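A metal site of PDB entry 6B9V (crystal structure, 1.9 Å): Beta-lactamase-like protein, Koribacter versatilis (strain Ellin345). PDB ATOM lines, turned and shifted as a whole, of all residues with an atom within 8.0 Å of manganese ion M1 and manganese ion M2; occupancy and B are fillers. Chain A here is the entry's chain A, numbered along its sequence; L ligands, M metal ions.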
ATOM      1  N   GLY A  13      14.343  -1.175 -26.733  1.00  0.00           N
ATOM      2  CA  GLY A  13      13.103  -0.524 -26.359  1.00  0.00           C
ATOM      3  C   GLY A  13      12.143  -1.387 -25.531  1.00  0.00           C
ATOM      4  O   GLY A  13      12.362  -2.570 -25.324  1.00  0.00           O
ATOM      5  N   THR A  14      11.075  -0.760 -25.064  1.00  0.00           N
ATOM      6  CA  THR A  14      10.043  -1.437 -24.295  1.00  0.00           C
ATOM      7  C   THR A  14       9.068  -2.212 -25.226  1.00  0.00           C
ATOM      8  O   THR A  14       9.300  -2.309 -26.444  1.00  0.00           O
ATOM      9  CB  THR A  14       9.249  -0.425 -23.414  1.00  0.00           C
ATOM     10  OG1 THR A  14       8.390  -1.152 -22.519  1.00  0.00           O
ATOM     11  CG2 THR A  14       8.422   0.545 -24.271  1.00  0.00           C
ATOM     12  N   SER A  15       7.988  -2.746 -24.648  1.00  0.00           N
ATOM     13  CA  SER A  15       7.138  -3.709 -25.377  1.00  0.00           C
ATOM     14  C   SER A  15       6.449  -3.092 -26.592  1.00  0.00           C
ATOM     15  O   SER A  15       6.236  -3.782 -27.592  1.00  0.00           O
ATOM     16  CB  SER A  15       6.086  -4.293 -24.430  1.00  0.00           C
ATOM     17  OG  SER A  15       5.215  -3.284 -23.973  1.00  0.00           O
ATOM     18  N   MET A  16       6.096  -1.831 -26.532  1.00  0.00           N
ATOM     19  CA  MET A  16       5.514  -1.156 -27.680  1.00  0.00           C
ATOM     20  C   MET A  16       6.552  -0.339 -28.497  1.00  0.00           C
ATOM     21  O   MET A  16       6.212   0.326 -29.435  1.00  0.00           O
ATOM     22  CB  MET A  16       4.354  -0.278 -27.234  1.00  0.00           C
ATOM     23  CG  MET A  16       3.079  -1.028 -26.888  1.00  0.00           C
ATOM     24  SD  MET A  16       2.329  -2.180 -28.164  1.00  0.00           S
ATOM     25  CE  MET A  16       2.299  -1.354 -29.817  1.00  0.00           C
ATOM     26  N   ARG A  39      11.969  -3.677 -30.265  1.00  0.00           N
ATOM     27  CA  ARG A  39      11.713  -4.465 -29.082  1.00  0.00           C
ATOM     28  C   ARG A  39      12.992  -5.194 -28.566  1.00  0.00           C
ATOM     29  O   ARG A  39      13.900  -5.366 -29.314  1.00  0.00           O
ATOM     30  CB  ARG A  39      10.529  -5.419 -29.276  1.00  0.00           C
ATOM     31  CG  ARG A  39       9.154  -4.822 -28.940  1.00  0.00           C
ATOM     32  CD  ARG A  39       8.825  -3.566 -29.690  1.00  0.00           C
ATOM     33  NE  ARG A  39       8.404  -3.801 -31.050  1.00  0.00           N
ATOM     34  CZ  ARG A  39       7.185  -4.048 -31.441  1.00  0.00           C
ATOM     35  NH1 ARG A  39       6.178  -4.095 -30.584  1.00  0.00           N
ATOM     36  NH2 ARG A  39       6.941  -4.287 -32.684  1.00  0.00           N
ATOM     37  N   PRO A  40      12.997  -5.602 -27.293  1.00  0.00           N
ATOM     38  CA  PRO A  40      14.288  -5.878 -26.650  1.00  0.00           C
ATOM     39  C   PRO A  40      14.915  -7.257 -26.887  1.00  0.00           C
ATOM     40  O   PRO A  40      14.287  -8.287 -26.649  1.00  0.00           O
ATOM     41  CB  PRO A  40      13.967  -5.675 -25.144  1.00  0.00           C
ATOM     42  CG  PRO A  40      12.524  -6.061 -25.009  1.00  0.00           C
ATOM     43  CD  PRO A  40      11.869  -5.605 -26.329  1.00  0.00           C
ATOM     44  N   ASP A  54      16.107 -14.037 -27.107  1.00  0.00           N
ATOM     45  CA  ASP A  54      14.706 -13.632 -27.375  1.00  0.00           C
ATOM     46  C   ASP A  54      14.450 -13.360 -28.863  1.00  0.00           C
ATOM     47  O   ASP A  54      15.328 -12.933 -29.600  1.00  0.00           O
ATOM     48  CB  ASP A  54      14.310 -12.411 -26.521  1.00  0.00           C
ATOM     49  CG  ASP A  54      14.126 -12.766 -25.038  1.00  0.00           C
ATOM     50  OD1 ASP A  54      13.969 -13.970 -24.730  1.00  0.00           O
ATOM     51  OD2 ASP A  54      14.122 -11.860 -24.190  1.00  0.00           O
ATOM     52  N   THR A  77      14.411 -15.398 -22.279  1.00  0.00           N
ATOM     53  CA  THR A  77      14.263 -14.897 -20.912  1.00  0.00           C
ATOM     54  C   THR A  77      12.886 -15.260 -20.318  1.00  0.00           C
ATOM     55  O   THR A  77      12.786 -15.683 -19.161  1.00  0.00           O
ATOM     56  CB  THR A  77      14.454 -13.355 -20.839  1.00  0.00           C
ATOM     57  OG1 THR A  77      13.478 -12.721 -21.682  1.00  0.00           O
ATOM     58  CG2 THR A  77      15.859 -12.953 -21.284  1.00  0.00           C
ATOM     59  N   HIS A  78      11.824 -15.093 -21.123  1.00  0.00           N
ATOM     60  CA  HIS A  78      10.457 -15.387 -20.688  1.00  0.00           C
ATOM     61  C   HIS A  78       9.513 -15.296 -21.879  1.00  0.00           C
ATOM     62  O   HIS A  78       9.939 -15.030 -23.001  1.00  0.00           O
ATOM     63  CB  HIS A  78       9.980 -14.444 -19.560  1.00  0.00           C
ATOM     64  CG  HIS A  78       9.831 -13.001 -19.947  1.00  0.00           C
ATOM     65  ND1 HIS A  78      10.856 -12.279 -20.551  1.00  0.00           N
ATOM     66  CD2 HIS A  78       8.819 -12.110 -19.772  1.00  0.00           C
ATOM     67  CE1 HIS A  78      10.463 -11.038 -20.735  1.00  0.00           C
ATOM     68  NE2 HIS A  78       9.234 -10.910 -20.274  1.00  0.00           N
ATOM     69  N   GLY A  79       8.225 -15.507 -21.617  1.00  0.00           N
ATOM     70  CA  GLY A  79       7.251 -15.737 -22.687  1.00  0.00           C
ATOM     71  C   GLY A  79       6.320 -14.616 -23.102  1.00  0.00           C
ATOM     72  O   GLY A  79       5.387 -14.846 -23.878  1.00  0.00           O
ATOM     73  N   HIS A  80       6.575 -13.402 -22.609  1.00  0.00           N
ATOM     74  CA  HIS A  80       5.780 -12.243 -23.023  1.00  0.00           C
ATOM     75  C   HIS A  80       5.915 -11.987 -24.521  1.00  0.00           C
ATOM     76  O   HIS A  80       6.919 -12.307 -25.139  1.00  0.00           O
ATOM     77  CB  HIS A  80       6.187 -11.001 -22.211  1.00  0.00           C
ATOM     78  CG  HIS A  80       5.638 -10.995 -20.816  1.00  0.00           C
ATOM     79  ND1 HIS A  80       6.118 -10.179 -19.824  1.00  0.00           N
ATOM     80  CD2 HIS A  80       4.631 -11.711 -20.268  1.00  0.00           C
ATOM     81  CE1 HIS A  80       5.443 -10.412 -18.704  1.00  0.00           C
ATOM     82  NE2 HIS A  80       4.533 -11.334 -18.944  1.00  0.00           N
ATOM     83  N   ALA A  81       4.866 -11.402 -25.098  1.00  0.00           N
ATOM     84  CA  ALA A  81       4.773 -11.218 -26.543  1.00  0.00           C
ATOM     85  C   ALA A  81       5.948 -10.463 -27.166  1.00  0.00           C
ATOM     86  O   ALA A  81       6.410 -10.837 -28.270  1.00  0.00           O
ATOM     87  CB  ALA A  81       3.463 -10.521 -26.873  1.00  0.00           C
ATOM     88  N   ASP A  82       6.437  -9.434 -26.478  1.00  0.00           N
ATOM     89  CA  ASP A  82       7.528  -8.640 -27.012  1.00  0.00           C
ATOM     90  C   ASP A  82       8.861  -9.405 -27.043  1.00  0.00           C
ATOM     91  O   ASP A  82       9.839  -8.895 -27.594  1.00  0.00           O
ATOM     92  CB  ASP A  82       7.697  -7.303 -26.249  1.00  0.00           C
ATOM     93  CG  ASP A  82       7.750  -7.455 -24.721  1.00  0.00           C
ATOM     94  OD1 ASP A  82       6.953  -8.217 -24.135  1.00  0.00           O
ATOM     95  OD2 ASP A  82       8.588  -6.766 -24.107  1.00  0.00           O
ATOM     96  N   HIS A  83       8.864 -10.636 -26.511  1.00  0.00           N
ATOM     97  CA  HIS A  83      10.064 -11.465 -26.477  1.00  0.00           C
ATOM     98  C   HIS A  83       9.943 -12.746 -27.305  1.00  0.00           C
ATOM     99  O   HIS A  83      10.931 -13.451 -27.493  1.00  0.00           O
ATOM    100  CB  HIS A  83      10.397 -11.819 -25.006  1.00  0.00           C
ATOM    101  CG  HIS A  83      10.625 -10.609 -24.155  1.00  0.00           C
ATOM    102  ND1 HIS A  83      11.889 -10.129 -23.859  1.00  0.00           N
ATOM    103  CD2 HIS A  83       9.755  -9.726 -23.603  1.00  0.00           C
ATOM    104  CE1 HIS A  83      11.784  -9.024 -23.151  1.00  0.00           C
ATOM    105  NE2 HIS A  83      10.498  -8.766 -22.963  1.00  0.00           N
ATOM    106  N   HIS A 160       9.881 -10.690 -12.085  1.00  0.00           N
ATOM    107  CA  HIS A 160       9.194  -9.871 -13.070  1.00  0.00           C
ATOM    108  C   HIS A 160       7.789  -9.713 -12.499  1.00  0.00           C
ATOM    109  O   HIS A 160       6.894 -10.507 -12.801  1.00  0.00           O
ATOM    110  CB  HIS A 160       9.220 -10.562 -14.451  1.00  0.00           C
ATOM    111  CG  HIS A 160       8.690  -9.746 -15.600  1.00  0.00           C
ATOM    112  ND1 HIS A 160       8.565  -8.375 -15.556  1.00  0.00           N
ATOM    113  CD2 HIS A 160       8.335 -10.130 -16.853  1.00  0.00           C
ATOM    114  CE1 HIS A 160       8.120  -7.938 -16.740  1.00  0.00           C
ATOM    115  NE2 HIS A 160       7.970  -8.973 -17.531  1.00  0.00           N
ATOM    116  N   ILE A 165      11.572 -15.194 -13.759  1.00  0.00           N
ATOM    117  CA  ILE A 165      12.050 -15.409 -15.134  1.00  0.00           C
ATOM    118  C   ILE A 165      13.584 -15.459 -15.085  1.00  0.00           C
ATOM    119  O   ILE A 165      14.170 -15.400 -14.002  1.00  0.00           O
ATOM    120  CB  ILE A 165      11.581 -14.291 -16.115  1.00  0.00           C
ATOM    121  CG1 ILE A 165      12.248 -12.957 -15.795  1.00  0.00           C
ATOM    122  CG2 ILE A 165      10.055 -14.159 -16.068  1.00  0.00           C
ATOM    123  CD1 ILE A 165      12.170 -11.936 -16.958  1.00  0.00           C
ATOM    124  N   THR A 177      16.772  -8.488 -18.288  1.00  0.00           N
ATOM    125  CA  THR A 177      15.702  -7.569 -18.679  1.00  0.00           C
ATOM    126  C   THR A 177      14.407  -7.968 -17.981  1.00  0.00           C
ATOM    127  O   THR A 177      14.326  -9.057 -17.414  1.00  0.00           O
ATOM    128  CB  THR A 177      15.503  -7.564 -20.216  1.00  0.00           C
ATOM    129  OG1 THR A 177      14.514  -6.577 -20.556  1.00  0.00           O
ATOM    130  CG2 THR A 177      15.069  -8.945 -20.723  1.00  0.00           C
ATOM    131  N   ASP A 178      13.416  -7.065 -17.994  1.00  0.00           N
ATOM    132  CA  ASP A 178      12.087  -7.368 -17.456  1.00  0.00           C
ATOM    133  C   ASP A 178      12.122  -7.852 -16.009  1.00  0.00           C
ATOM    134  O   ASP A 178      11.648  -8.949 -15.692  1.00  0.00           O
ATOM    135  CB  ASP A 178      11.366  -8.416 -18.318  1.00  0.00           C
ATOM    136  CG  ASP A 178      11.002  -7.891 -19.720  1.00  0.00           C
ATOM    137  OD1 ASP A 178       9.810  -7.721 -20.023  1.00  0.00           O
ATOM    138  OD2 ASP A 178      11.930  -7.650 -20.498  1.00  0.00           O
ATOM    139  N   PHE A 179      12.711  -7.060 -15.122  1.00  0.00           N
ATOM    140  CA  PHE A 179      12.622  -7.405 -13.715  1.00  0.00           C
ATOM    141  C   PHE A 179      12.176  -6.200 -12.922  1.00  0.00           C
ATOM    142  O   PHE A 179      12.459  -5.058 -13.307  1.00  0.00           O
ATOM    143  CB  PHE A 179      13.959  -7.914 -13.147  1.00  0.00           C
ATOM    144  CG  PHE A 179      15.046  -6.876 -13.122  1.00  0.00           C
ATOM    145  CD1 PHE A 179      15.165  -5.996 -12.041  1.00  0.00           C
ATOM    146  CD2 PHE A 179      15.964  -6.782 -14.164  1.00  0.00           C
ATOM    147  CE1 PHE A 179      16.159  -5.026 -12.024  1.00  0.00           C
ATOM    148  CE2 PHE A 179      16.976  -5.821 -14.142  1.00  0.00           C
ATOM    149  CZ  PHE A 179      17.061  -4.926 -13.080  1.00  0.00           C
ATOM    150  N   ASP A 199      17.278  -3.836 -16.956  1.00  0.00           N
ATOM    151  CA  ASP A 199      15.989  -3.179 -17.226  1.00  0.00           C
ATOM    152  C   ASP A 199      15.964  -1.756 -16.657  1.00  0.00           C
ATOM    153  O   ASP A 199      16.315  -1.552 -15.492  1.00  0.00           O
ATOM    154  CB  ASP A 199      14.888  -4.053 -16.594  1.00  0.00           C
ATOM    155  CG  ASP A 199      13.481  -3.530 -16.823  1.00  0.00           C
ATOM    156  OD1 ASP A 199      13.096  -2.506 -16.234  1.00  0.00           O
ATOM    157  OD2 ASP A 199      12.740  -4.179 -17.592  1.00  0.00           O
ATOM    158  N   LEU A 201      12.863   1.013 -17.333  1.00  0.00           N
ATOM    159  CA  LEU A 201      11.706   1.320 -18.156  1.00  0.00           C
ATOM    160  C   LEU A 201      11.425   2.814 -18.245  1.00  0.00           C
ATOM    161  O   LEU A 201      11.154   3.341 -19.329  1.00  0.00           O
ATOM    162  CB  LEU A 201      10.472   0.608 -17.618  1.00  0.00           C
ATOM    163  CG  LEU A 201       9.135   0.908 -18.305  1.00  0.00           C
ATOM    164  CD1 LEU A 201       9.125   0.244 -19.710  1.00  0.00           C
ATOM    165  CD2 LEU A 201       7.952   0.420 -17.458  1.00  0.00           C
ATOM    166  N   THR A 208       6.107  -4.230 -12.757  1.00  0.00           N
ATOM    167  CA  THR A 208       6.881  -5.381 -13.224  1.00  0.00           C
ATOM    168  C   THR A 208       8.238  -5.025 -13.805  1.00  0.00           C
ATOM    169  O   THR A 208       8.971  -5.917 -14.251  1.00  0.00           O
ATOM    170  CB  THR A 208       6.094  -6.214 -14.286  1.00  0.00           C
ATOM    171  OG1 THR A 208       5.815  -5.404 -15.424  1.00  0.00           O
ATOM    172  CG2 THR A 208       4.778  -6.732 -13.702  1.00  0.00           C
ATOM    173  N   HIS A 209       8.591  -3.735 -13.794  1.00  0.00           N
ATOM    174  CA  HIS A 209       9.862  -3.293 -14.359  1.00  0.00           C
ATOM    175  C   HIS A 209      10.622  -2.474 -13.314  1.00  0.00           C
ATOM    176  O   HIS A 209      10.128  -2.266 -12.207  1.00  0.00           O
ATOM    177  CB  HIS A 209       9.650  -2.502 -15.659  1.00  0.00           C
ATOM    178  CG  HIS A 209       9.213  -3.359 -16.817  1.00  0.00           C
ATOM    179  ND1 HIS A 209      10.117  -3.978 -17.661  1.00  0.00           N
ATOM    180  CD2 HIS A 209       7.980  -3.710 -17.273  1.00  0.00           C
ATOM    181  CE1 HIS A 209       9.472  -4.668 -18.571  1.00  0.00           C
ATOM    182  NE2 HIS A 209       8.171  -4.520 -18.371  1.00  0.00           N
ATOM    183  N   HIS A 231      15.176  -2.056 -22.392  1.00  0.00           N
ATOM    184  CA  HIS A 231      13.710  -2.107 -22.235  1.00  0.00           C
ATOM    185  C   HIS A 231      13.142  -0.694 -21.976  1.00  0.00           C
ATOM    186  O   HIS A 231      12.170  -0.506 -21.259  1.00  0.00           O
ATOM    187  CB  HIS A 231      13.300  -3.057 -21.110  1.00  0.00           C
ATOM    188  CG  HIS A 231      11.995  -3.737 -21.346  1.00  0.00           C
ATOM    189  ND1 HIS A 231      10.787  -3.069 -21.325  1.00  0.00           N
ATOM    190  CD2 HIS A 231      11.696  -5.022 -21.639  1.00  0.00           C
ATOM    191  CE1 HIS A 231       9.805  -3.914 -21.578  1.00  0.00           C
ATOM    192  NE2 HIS A 231      10.328  -5.104 -21.790  1.00  0.00           N
HETATM  193  P1  LIG L   1       6.702  -6.737 -20.772  1.00  0.00           P
HETATM  194  O1  LIG L   1       7.537  -7.832 -21.444  1.00  0.00           O
HETATM  195  O2  LIG L   1       7.326  -5.393 -20.978  1.00  0.00           O
HETATM  196  O3  LIG L   1       6.626  -6.996 -19.281  1.00  0.00           O
HETATM  197  O4  LIG L   1       5.309  -6.719 -21.377  1.00  0.00           O
HETATM  198 MN    MN M   1       7.902  -9.175 -19.768  1.00  0.00          MN
HETATM  199 MN    MN M   2       9.445  -7.065 -22.085  1.00  0.00          MN
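ND1 of His 83 is in hydrogen-bond range of OD2 of Asp 54. The side-chain hydroxyl of Thr 14 sits close to a ring nitrogen (ND1) of His 231 (3.3 Å). The side-chain carboxylate of Asp 178 is in hydrogen-bond range of the side-chain hydroxyl of Thr 177, 2.8 Å away. A ring nitrogen (ND1) of His 78 is in hydrogen-bond range of the side-chain hydroxyl of Thr 77, at 2.9 Å. ND1 of His 160 lies within hydrogen-bond range of O of Thr 208, 2.8 Å away. The side-chain carboxylate (OD2) of Asp 199 sits at hydrogen-bond distance from the backbone NH (N) of Asp 178 (3.0 Å).
Four residues have an atom within 4 Å of manganese ion M1: His 78, His 80, His 160 and Asp 178. The nearest printed residue that does not touch manganese ion M1 is His 83 (4.1 Å).
Four residues have an atom within 4 Å of manganese ion M2: Asp 82, His 83, Asp 178 and His 231. The nearest printed residue that does not touch manganese ion M2 is His 209 (4.3 Å).
ND1 of His 80 is bound to manganese ion M1 (2.0 Å). Manganese ion M1 is bound by O1 of the ligand, 2.2 Å away. Manganese ion M1 is bound by NE2 of His 78 (2.2 Å). A ring nitrogen (NE2) of His 160 binds manganese ion M1, at 2.2 Å. Manganese ion M1 is bound by OD1 of Asp 178. O3 of the ligand binds manganese ion M1, at 2.6 Å. Manganese ion M1 has six donor atoms within binding distance.
Manganese ion M2 is bound by an oxygen (O1) of the ligand (2.2 Å), a ring nitrogen (NE2) of His 231 (2.2 Å), a ring nitrogen (NE2) of His 83 (2.2 Å), the side-chain carboxylate (OD1) of Asp 178 (2.2 Å) and the side-chain carboxylate (OD2) of Asp 82 (2.2 Å). Slightly farther from manganese ion M2 lies an oxygen (O2) of the ligand (2.9 Å).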
